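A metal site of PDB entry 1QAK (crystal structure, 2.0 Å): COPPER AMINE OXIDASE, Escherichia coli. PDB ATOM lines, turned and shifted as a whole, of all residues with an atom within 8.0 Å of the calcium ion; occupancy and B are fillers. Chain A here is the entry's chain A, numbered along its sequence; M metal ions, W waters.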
ATOM      1  N   LYS A 128       0.221 -17.887  -9.990  1.00  0.00           N
ATOM      2  CA  LYS A 128      -0.135 -18.576  -8.751  1.00  0.00           C
ATOM      3  C   LYS A 128      -1.629 -18.809  -8.542  1.00  0.00           C
ATOM      4  O   LYS A 128      -2.125 -19.875  -8.162  1.00  0.00           O
ATOM      5  CB  LYS A 128       0.490 -17.709  -7.665  1.00  0.00           C
ATOM      6  CG  LYS A 128      -0.066 -17.816  -6.256  1.00  0.00           C
ATOM      7  CD  LYS A 128       0.938 -17.295  -5.195  1.00  0.00           C
ATOM      8  CE  LYS A 128       0.449 -17.740  -3.815  1.00  0.00           C
ATOM      9  NZ  LYS A 128       1.377 -17.199  -2.748  1.00  0.00           N
ATOM     10  N   TRP A 132      -3.397 -22.442  -7.990  1.00  0.00           N
ATOM     11  CA  TRP A 132      -4.235 -22.761  -6.842  1.00  0.00           C
ATOM     12  C   TRP A 132      -5.646 -23.181  -7.302  1.00  0.00           C
ATOM     13  O   TRP A 132      -6.176 -24.126  -6.724  1.00  0.00           O
ATOM     14  CB  TRP A 132      -4.382 -21.647  -5.811  1.00  0.00           C
ATOM     15  CG  TRP A 132      -3.429 -21.613  -4.657  1.00  0.00           C
ATOM     16  CD1 TRP A 132      -2.700 -20.540  -4.223  1.00  0.00           C
ATOM     17  CD2 TRP A 132      -3.134 -22.688  -3.759  1.00  0.00           C
ATOM     18  NE1 TRP A 132      -1.925 -20.871  -3.127  1.00  0.00           N
ATOM     19  CE2 TRP A 132      -2.205 -22.197  -2.826  1.00  0.00           C
ATOM     20  CE3 TRP A 132      -3.572 -24.015  -3.688  1.00  0.00           C
ATOM     21  CZ2 TRP A 132      -1.677 -23.012  -1.801  1.00  0.00           C
ATOM     22  CZ3 TRP A 132      -3.048 -24.801  -2.653  1.00  0.00           C
ATOM     23  CH2 TRP A 132      -2.130 -24.319  -1.730  1.00  0.00           C
ATOM     24  N   VAL A 351      -1.956 -24.229   2.849  1.00  0.00           N
ATOM     25  CA  VAL A 351      -0.902 -24.178   3.843  1.00  0.00           C
ATOM     26  C   VAL A 351       0.310 -23.466   3.192  1.00  0.00           C
ATOM     27  O   VAL A 351       0.765 -22.427   3.682  1.00  0.00           O
ATOM     28  CB  VAL A 351      -0.537 -25.546   4.426  1.00  0.00           C
ATOM     29  CG1 VAL A 351       0.684 -25.500   5.353  1.00  0.00           C
ATOM     30  CG2 VAL A 351      -1.692 -26.126   5.236  1.00  0.00           C
ATOM     31  N   MET A 352       0.776 -24.070   2.094  1.00  0.00           N
ATOM     32  CA  MET A 352       1.916 -23.570   1.347  1.00  0.00           C
ATOM     33  C   MET A 352       1.761 -23.686  -0.160  1.00  0.00           C
ATOM     34  O   MET A 352       1.514 -24.757  -0.728  1.00  0.00           O
ATOM     35  CB  MET A 352       3.151 -24.358   1.851  1.00  0.00           C
ATOM     36  CG  MET A 352       4.485 -23.858   1.276  1.00  0.00           C
ATOM     37  SD  MET A 352       5.990 -24.436   2.094  1.00  0.00           S
ATOM     38  CE  MET A 352       5.772 -26.188   1.676  1.00  0.00           C
ATOM     39  N   TYR A 353       1.920 -22.576  -0.879  1.00  0.00           N
ATOM     40  CA  TYR A 353       1.854 -22.553  -2.345  1.00  0.00           C
ATOM     41  C   TYR A 353       3.170 -23.164  -2.844  1.00  0.00           C
ATOM     42  O   TYR A 353       3.129 -24.029  -3.737  1.00  0.00           O
ATOM     43  CB  TYR A 353       1.748 -21.113  -2.914  1.00  0.00           C
ATOM     44  CG  TYR A 353       1.787 -21.198  -4.430  1.00  0.00           C
ATOM     45  CD1 TYR A 353       0.759 -21.842  -5.100  1.00  0.00           C
ATOM     46  CD2 TYR A 353       2.849 -20.658  -5.147  1.00  0.00           C
ATOM     47  CE1 TYR A 353       0.775 -21.939  -6.494  1.00  0.00           C
ATOM     48  CE2 TYR A 353       2.905 -20.740  -6.537  1.00  0.00           C
ATOM     49  CZ  TYR A 353       1.858 -21.386  -7.166  1.00  0.00           C
ATOM     50  OH  TYR A 353       1.794 -21.545  -8.520  1.00  0.00           O
ATOM     51  N   GLU A 354       4.349 -22.802  -2.340  1.00  0.00           N
ATOM     52  CA  GLU A 354       5.597 -23.412  -2.846  1.00  0.00           C
ATOM     53  C   GLU A 354       6.642 -23.287  -1.729  1.00  0.00           C
ATOM     54  O   GLU A 354       6.689 -22.253  -1.062  1.00  0.00           O
ATOM     55  CB  GLU A 354       6.318 -22.744  -4.027  1.00  0.00           C
ATOM     56  CG  GLU A 354       5.480 -22.610  -5.279  1.00  0.00           C
ATOM     57  CD  GLU A 354       6.178 -21.766  -6.340  1.00  0.00           C
ATOM     58  OE1 GLU A 354       6.613 -22.456  -7.264  1.00  0.00           O
ATOM     59  OE2 GLU A 354       6.298 -20.528  -6.309  1.00  0.00           O
ATOM     60  N   ARG A 526      13.068 -21.102   1.258  1.00  0.00           N
ATOM     61  CA  ARG A 526      12.080 -20.143   0.757  1.00  0.00           C
ATOM     62  C   ARG A 526      10.758 -20.868   0.894  1.00  0.00           C
ATOM     63  O   ARG A 526      10.498 -21.906   0.252  1.00  0.00           O
ATOM     64  CB  ARG A 526      12.297 -19.850  -0.740  1.00  0.00           C
ATOM     65  CG  ARG A 526      11.207 -18.925  -1.309  1.00  0.00           C
ATOM     66  CD  ARG A 526      11.477 -18.690  -2.823  1.00  0.00           C
ATOM     67  NE  ARG A 526      10.427 -17.756  -3.285  1.00  0.00           N
ATOM     68  CZ  ARG A 526       9.202 -18.140  -3.625  1.00  0.00           C
ATOM     69  NH1 ARG A 526       8.886 -19.439  -3.590  1.00  0.00           N
ATOM     70  NH2 ARG A 526       8.277 -17.257  -4.022  1.00  0.00           N
ATOM     71  N   LEU A 527       9.904 -20.295   1.750  1.00  0.00           N
ATOM     72  CA  LEU A 527       8.600 -20.898   2.019  1.00  0.00           C
ATOM     73  C   LEU A 527       7.424 -19.984   1.745  1.00  0.00           C
ATOM     74  O   LEU A 527       7.073 -19.144   2.571  1.00  0.00           O
ATOM     75  CB  LEU A 527       8.555 -21.370   3.512  1.00  0.00           C
ATOM     76  CG  LEU A 527       9.778 -22.251   3.873  1.00  0.00           C
ATOM     77  CD1 LEU A 527       9.918 -22.286   5.396  1.00  0.00           C
ATOM     78  CD2 LEU A 527       9.748 -23.623   3.208  1.00  0.00           C
ATOM     79  N   ASP A 528       6.812 -20.145   0.598  1.00  0.00           N
ATOM     80  CA  ASP A 528       5.657 -19.310   0.251  1.00  0.00           C
ATOM     81  C   ASP A 528       4.433 -19.880   0.962  1.00  0.00           C
ATOM     82  O   ASP A 528       3.589 -20.493   0.303  1.00  0.00           O
ATOM     83  CB  ASP A 528       5.471 -19.195  -1.250  1.00  0.00           C
ATOM     84  CG  ASP A 528       4.275 -18.350  -1.601  1.00  0.00           C
ATOM     85  OD1 ASP A 528       3.688 -17.758  -0.695  1.00  0.00           O
ATOM     86  OD2 ASP A 528       3.877 -18.245  -2.761  1.00  0.00           O
ATOM     87  N   LEU A 529       4.366 -19.646   2.284  1.00  0.00           N
ATOM     88  CA  LEU A 529       3.222 -20.139   3.049  1.00  0.00           C
ATOM     89  C   LEU A 529       1.983 -19.296   2.689  1.00  0.00           C
ATOM     90  O   LEU A 529       2.207 -18.103   2.598  1.00  0.00           O
ATOM     91  CB  LEU A 529       3.425 -19.913   4.578  1.00  0.00           C
ATOM     92  CG  LEU A 529       4.570 -20.794   5.120  1.00  0.00           C
ATOM     93  CD1 LEU A 529       5.049 -20.419   6.511  1.00  0.00           C
ATOM     94  CD2 LEU A 529       4.197 -22.287   5.066  1.00  0.00           C
ATOM     95  N   ASP A 530       0.800 -19.848   2.543  1.00  0.00           N
ATOM     96  CA  ASP A 530      -0.433 -19.099   2.236  1.00  0.00           C
ATOM     97  C   ASP A 530      -1.301 -19.717   3.347  1.00  0.00           C
ATOM     98  O   ASP A 530      -1.953 -20.744   3.103  1.00  0.00           O
ATOM     99  CB  ASP A 530      -1.062 -19.516   0.903  1.00  0.00           C
ATOM    100  CG  ASP A 530      -0.443 -18.776  -0.268  1.00  0.00           C
ATOM    101  OD1 ASP A 530       0.389 -17.877  -0.080  1.00  0.00           O
ATOM    102  OD2 ASP A 530      -0.764 -19.113  -1.423  1.00  0.00           O
ATOM    103  N   VAL A 531      -1.256 -19.090   4.532  1.00  0.00           N
ATOM    104  CA  VAL A 531      -2.007 -19.640   5.656  1.00  0.00           C
ATOM    105  C   VAL A 531      -3.515 -19.512   5.530  1.00  0.00           C
ATOM    106  O   VAL A 531      -4.050 -18.449   5.869  1.00  0.00           O
ATOM    107  CB  VAL A 531      -1.468 -19.057   6.985  1.00  0.00           C
ATOM    108  CG1 VAL A 531      -2.293 -19.673   8.106  1.00  0.00           C
ATOM    109  CG2 VAL A 531      -0.025 -19.492   7.146  1.00  0.00           C
ATOM    110  N   GLY A 533      -5.130 -19.097   3.002  1.00  0.00           N
ATOM    111  CA  GLY A 533      -5.517 -18.055   2.016  1.00  0.00           C
ATOM    112  C   GLY A 533      -4.245 -17.281   1.745  1.00  0.00           C
ATOM    113  O   GLY A 533      -3.231 -17.456   2.445  1.00  0.00           O
ATOM    114  N   GLU A 534      -4.285 -16.439   0.731  1.00  0.00           N
ATOM    115  CA  GLU A 534      -3.162 -15.626   0.305  1.00  0.00           C
ATOM    116  C   GLU A 534      -2.816 -14.499   1.265  1.00  0.00           C
ATOM    117  O   GLU A 534      -1.675 -14.232   1.655  1.00  0.00           O
ATOM    118  CB  GLU A 534      -3.456 -15.053  -1.117  1.00  0.00           C
ATOM    119  CG  GLU A 534      -2.756 -15.765  -2.266  1.00  0.00           C
ATOM    120  CD  GLU A 534      -3.113 -17.048  -3.007  1.00  0.00           C
ATOM    121  OE1 GLU A 534      -3.310 -18.043  -2.246  1.00  0.00           O
ATOM    122  OE2 GLU A 534      -3.203 -17.173  -4.293  1.00  0.00           O
ATOM    123  N   ASN A 535      -3.814 -13.751   1.709  1.00  0.00           N
ATOM    124  CA  ASN A 535      -3.607 -12.614   2.597  1.00  0.00           C
ATOM    125  C   ASN A 535      -3.327 -12.910   4.054  1.00  0.00           C
ATOM    126  O   ASN A 535      -4.198 -13.322   4.810  1.00  0.00           O
ATOM    127  CB  ASN A 535      -4.867 -11.726   2.435  1.00  0.00           C
ATOM    128  CG  ASN A 535      -4.926 -11.193   1.001  1.00  0.00           C
ATOM    129  OD1 ASN A 535      -3.975 -10.953   0.294  1.00  0.00           O
ATOM    130  ND2 ASN A 535      -6.128 -10.975   0.502  1.00  0.00           N
ATOM    131  N   ASN A 536      -2.096 -12.687   4.463  1.00  0.00           N
ATOM    132  CA  ASN A 536      -1.626 -12.918   5.818  1.00  0.00           C
ATOM    133  C   ASN A 536      -0.843 -11.763   6.398  1.00  0.00           C
ATOM    134  O   ASN A 536      -0.533 -10.852   5.645  1.00  0.00           O
ATOM    135  CB  ASN A 536      -0.579 -14.074   5.693  1.00  0.00           C
ATOM    136  CG  ASN A 536      -1.214 -15.357   5.159  1.00  0.00           C
ATOM    137  OD1 ASN A 536      -2.453 -15.550   5.093  1.00  0.00           O
ATOM    138  ND2 ASN A 536      -0.346 -16.302   4.766  1.00  0.00           N
ATOM    139  N   LEU A 583       2.684 -16.518  11.229  1.00  0.00           N
ATOM    140  CA  LEU A 583       2.262 -16.073   9.895  1.00  0.00           C
ATOM    141  C   LEU A 583       0.771 -16.343  10.143  1.00  0.00           C
ATOM    142  O   LEU A 583       0.296 -17.480  10.191  1.00  0.00           O
ATOM    143  CB  LEU A 583       2.831 -16.729   8.645  1.00  0.00           C
ATOM    144  CG  LEU A 583       2.323 -15.967   7.389  1.00  0.00           C
ATOM    145  CD1 LEU A 583       2.968 -14.588   7.405  1.00  0.00           C
ATOM    146  CD2 LEU A 583       2.819 -16.668   6.128  1.00  0.00           C
ATOM    147  N   VAL A 635      10.711 -12.056   5.784  1.00  0.00           N
ATOM    148  CA  VAL A 635       9.358 -12.177   5.245  1.00  0.00           C
ATOM    149  C   VAL A 635       9.324 -11.068   4.187  1.00  0.00           C
ATOM    150  O   VAL A 635       9.639  -9.893   4.462  1.00  0.00           O
ATOM    151  CB  VAL A 635       8.213 -12.049   6.249  1.00  0.00           C
ATOM    152  CG1 VAL A 635       6.886 -12.329   5.573  1.00  0.00           C
ATOM    153  CG2 VAL A 635       8.504 -12.945   7.439  1.00  0.00           C
ATOM    154  N   THR A 636       8.970 -11.397   2.954  1.00  0.00           N
ATOM    155  CA  THR A 636       8.922 -10.391   1.880  1.00  0.00           C
ATOM    156  C   THR A 636       7.602 -10.638   1.168  1.00  0.00           C
ATOM    157  O   THR A 636       6.898 -11.662   1.289  1.00  0.00           O
ATOM    158  CB  THR A 636      10.057 -10.650   0.851  1.00  0.00           C
ATOM    159  OG1 THR A 636       9.854 -11.973   0.311  1.00  0.00           O
ATOM    160  CG2 THR A 636      11.449 -10.639   1.490  1.00  0.00           C
ATOM    161  N   ARG A 637       7.223  -9.635   0.391  1.00  0.00           N
ATOM    162  CA  ARG A 637       5.971  -9.702  -0.380  1.00  0.00           C
ATOM    163  C   ARG A 637       6.182 -10.687  -1.537  1.00  0.00           C
ATOM    164  O   ARG A 637       7.263 -10.671  -2.116  1.00  0.00           O
ATOM    165  CB  ARG A 637       5.570  -8.328  -0.929  1.00  0.00           C
ATOM    166  CG  ARG A 637       4.406  -8.587  -1.875  1.00  0.00           C
ATOM    167  CD  ARG A 637       3.048  -8.768  -1.174  1.00  0.00           C
ATOM    168  NE  ARG A 637       2.458  -7.460  -0.952  1.00  0.00           N
ATOM    169  CZ  ARG A 637       2.825  -6.183  -0.964  1.00  0.00           C
ATOM    170  NH1 ARG A 637       4.071  -5.816  -1.226  1.00  0.00           N
ATOM    171  NH2 ARG A 637       1.883  -5.298  -0.675  1.00  0.00           N
ATOM    172  N   TYR A 638       5.184 -11.516  -1.842  1.00  0.00           N
ATOM    173  CA  TYR A 638       5.362 -12.472  -2.920  1.00  0.00           C
ATOM    174  C   TYR A 638       5.613 -11.815  -4.272  1.00  0.00           C
ATOM    175  O   TYR A 638       4.871 -10.891  -4.618  1.00  0.00           O
ATOM    176  CB  TYR A 638       4.084 -13.290  -3.111  1.00  0.00           C
ATOM    177  CG  TYR A 638       4.070 -14.152  -4.356  1.00  0.00           C
ATOM    178  CD1 TYR A 638       4.814 -15.318  -4.442  1.00  0.00           C
ATOM    179  CD2 TYR A 638       3.277 -13.773  -5.443  1.00  0.00           C
ATOM    180  CE1 TYR A 638       4.821 -16.103  -5.580  1.00  0.00           C
ATOM    181  CE2 TYR A 638       3.284 -14.558  -6.582  1.00  0.00           C
ATOM    182  CZ  TYR A 638       4.044 -15.707  -6.660  1.00  0.00           C
ATOM    183  OH  TYR A 638       4.019 -16.485  -7.798  1.00  0.00           O
ATOM    184  N   THR A 672      -1.234  -9.265   3.389  1.00  0.00           N
ATOM    185  CA  THR A 672      -0.875  -9.427   1.977  1.00  0.00           C
ATOM    186  C   THR A 672      -0.195 -10.779   1.774  1.00  0.00           C
ATOM    187  O   THR A 672       0.121 -11.510   2.722  1.00  0.00           O
ATOM    188  CB  THR A 672      -0.025  -8.198   1.617  1.00  0.00           C
ATOM    189  OG1 THR A 672       0.111  -8.180   0.194  1.00  0.00           O
ATOM    190  CG2 THR A 672       1.291  -8.213   2.349  1.00  0.00           C
ATOM    191  N   ASP A 673       0.047 -11.143   0.540  1.00  0.00           N
ATOM    192  CA  ASP A 673       0.697 -12.408   0.170  1.00  0.00           C
ATOM    193  C   ASP A 673       2.148 -12.365   0.622  1.00  0.00           C
ATOM    194  O   ASP A 673       2.982 -11.689   0.024  1.00  0.00           O
ATOM    195  CB  ASP A 673       0.562 -12.663  -1.329  1.00  0.00           C
ATOM    196  CG  ASP A 673       0.972 -14.084  -1.682  1.00  0.00           C
ATOM    197  OD1 ASP A 673       1.497 -14.826  -0.822  1.00  0.00           O
ATOM    198  OD2 ASP A 673       0.798 -14.536  -2.829  1.00  0.00           O
ATOM    199  N   ALA A 674       2.488 -13.113   1.684  1.00  0.00           N
ATOM    200  CA  ALA A 674       3.858 -13.129   2.184  1.00  0.00           C
ATOM    201  C   ALA A 674       4.696 -14.375   1.832  1.00  0.00           C
ATOM    202  O   ALA A 674       4.112 -15.403   1.594  1.00  0.00           O
ATOM    203  CB  ALA A 674       3.814 -13.119   3.719  1.00  0.00           C
ATOM    204  N   VAL A 675       6.014 -14.263   1.853  1.00  0.00           N
ATOM    205  CA  VAL A 675       6.841 -15.453   1.552  1.00  0.00           C
ATOM    206  C   VAL A 675       7.821 -15.423   2.748  1.00  0.00           C
ATOM    207  O   VAL A 675       8.473 -14.396   2.992  1.00  0.00           O
ATOM    208  CB  VAL A 675       7.651 -15.305   0.246  1.00  0.00           C
ATOM    209  CG1 VAL A 675       8.570 -16.521   0.035  1.00  0.00           C
ATOM    210  CG2 VAL A 675       6.670 -15.214  -0.935  1.00  0.00           C
ATOM    211  N   VAL A 676       7.894 -16.528   3.480  1.00  0.00           N
ATOM    212  CA  VAL A 676       8.807 -16.606   4.616  1.00  0.00           C
ATOM    213  C   VAL A 676      10.167 -17.187   4.182  1.00  0.00           C
ATOM    214  O   VAL A 676      10.138 -18.102   3.346  1.00  0.00           O
ATOM    215  CB  VAL A 676       8.221 -17.587   5.663  1.00  0.00           C
ATOM    216  CG1 VAL A 676       9.182 -17.787   6.839  1.00  0.00           C
ATOM    217  CG2 VAL A 676       6.895 -17.064   6.208  1.00  0.00           C
HETATM  218 CA    CA M   1       2.207 -16.556   0.738  1.00  0.00          CA
HETATM  219  O   HOH W   1       0.595 -15.332   2.331  1.00  0.00           O
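OD2 of Asp 528 lies within salt-bridge range of NZ of Lys 128. The backbone carbonyl oxygen of Asp 528 sits at hydrogen-bond distance from the backbone NH of Tyr 353, at 2.9 Å. O of Glu 354 is in hydrogen-bond range of N of Asp 528. The side-chain carboxylate (OD2) of Asp 530 is in salt-bridge range of the side-chain amino group (NZ) of Lys 128, at 3.2 Å. N of Asp 530 is in hydrogen-bond range of O of Val 351. The indole nitrogen (NE1) of Trp 132 sits at hydrogen-bond distance from the side-chain carboxylate (OD2) of Asp 530, 2.7 Å away. The side-chain carboxylate (OD2) of Asp 673 lies within salt-bridge range of the side-chain amino group (NZ) of Lys 128. The backbone carbonyl oxygen (O) of Asp 673 lies within hydrogen-bond range of the backbone NH (N) of Tyr 638 (2.9 Å).
O of Ala 674 is bound to the calcium ion (2.4 Å). The calcium ion is bound by OD1 of Asp 528 (2.4 Å). The calcium ion is bound by OD1 of Asp 530 (2.4 Å). O of Leu 529 binds the calcium ion (2.4 Å). The side-chain carboxylate (OD1) of Asp 673 is bound to the calcium ion. The calcium ion is bound by water W1, 2.6 Å away.
Residues that only touch the calcium ion: Lys 128 (3.6 Å). Within 4 Å of the calcium ion: Lys 128, Asp 528, Leu 529, Asp 530, Asp 673 and Ala 674.
Water W1 lies within hydrogen-bond range of the backbone carbonyl oxygen (O) of Glu 534 (2.6 Å), the side-chain amide nitrogen (ND2) of Asn 536 (2.8 Å) and the backbone NH (N) of Ala 674 (3.0 Å).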
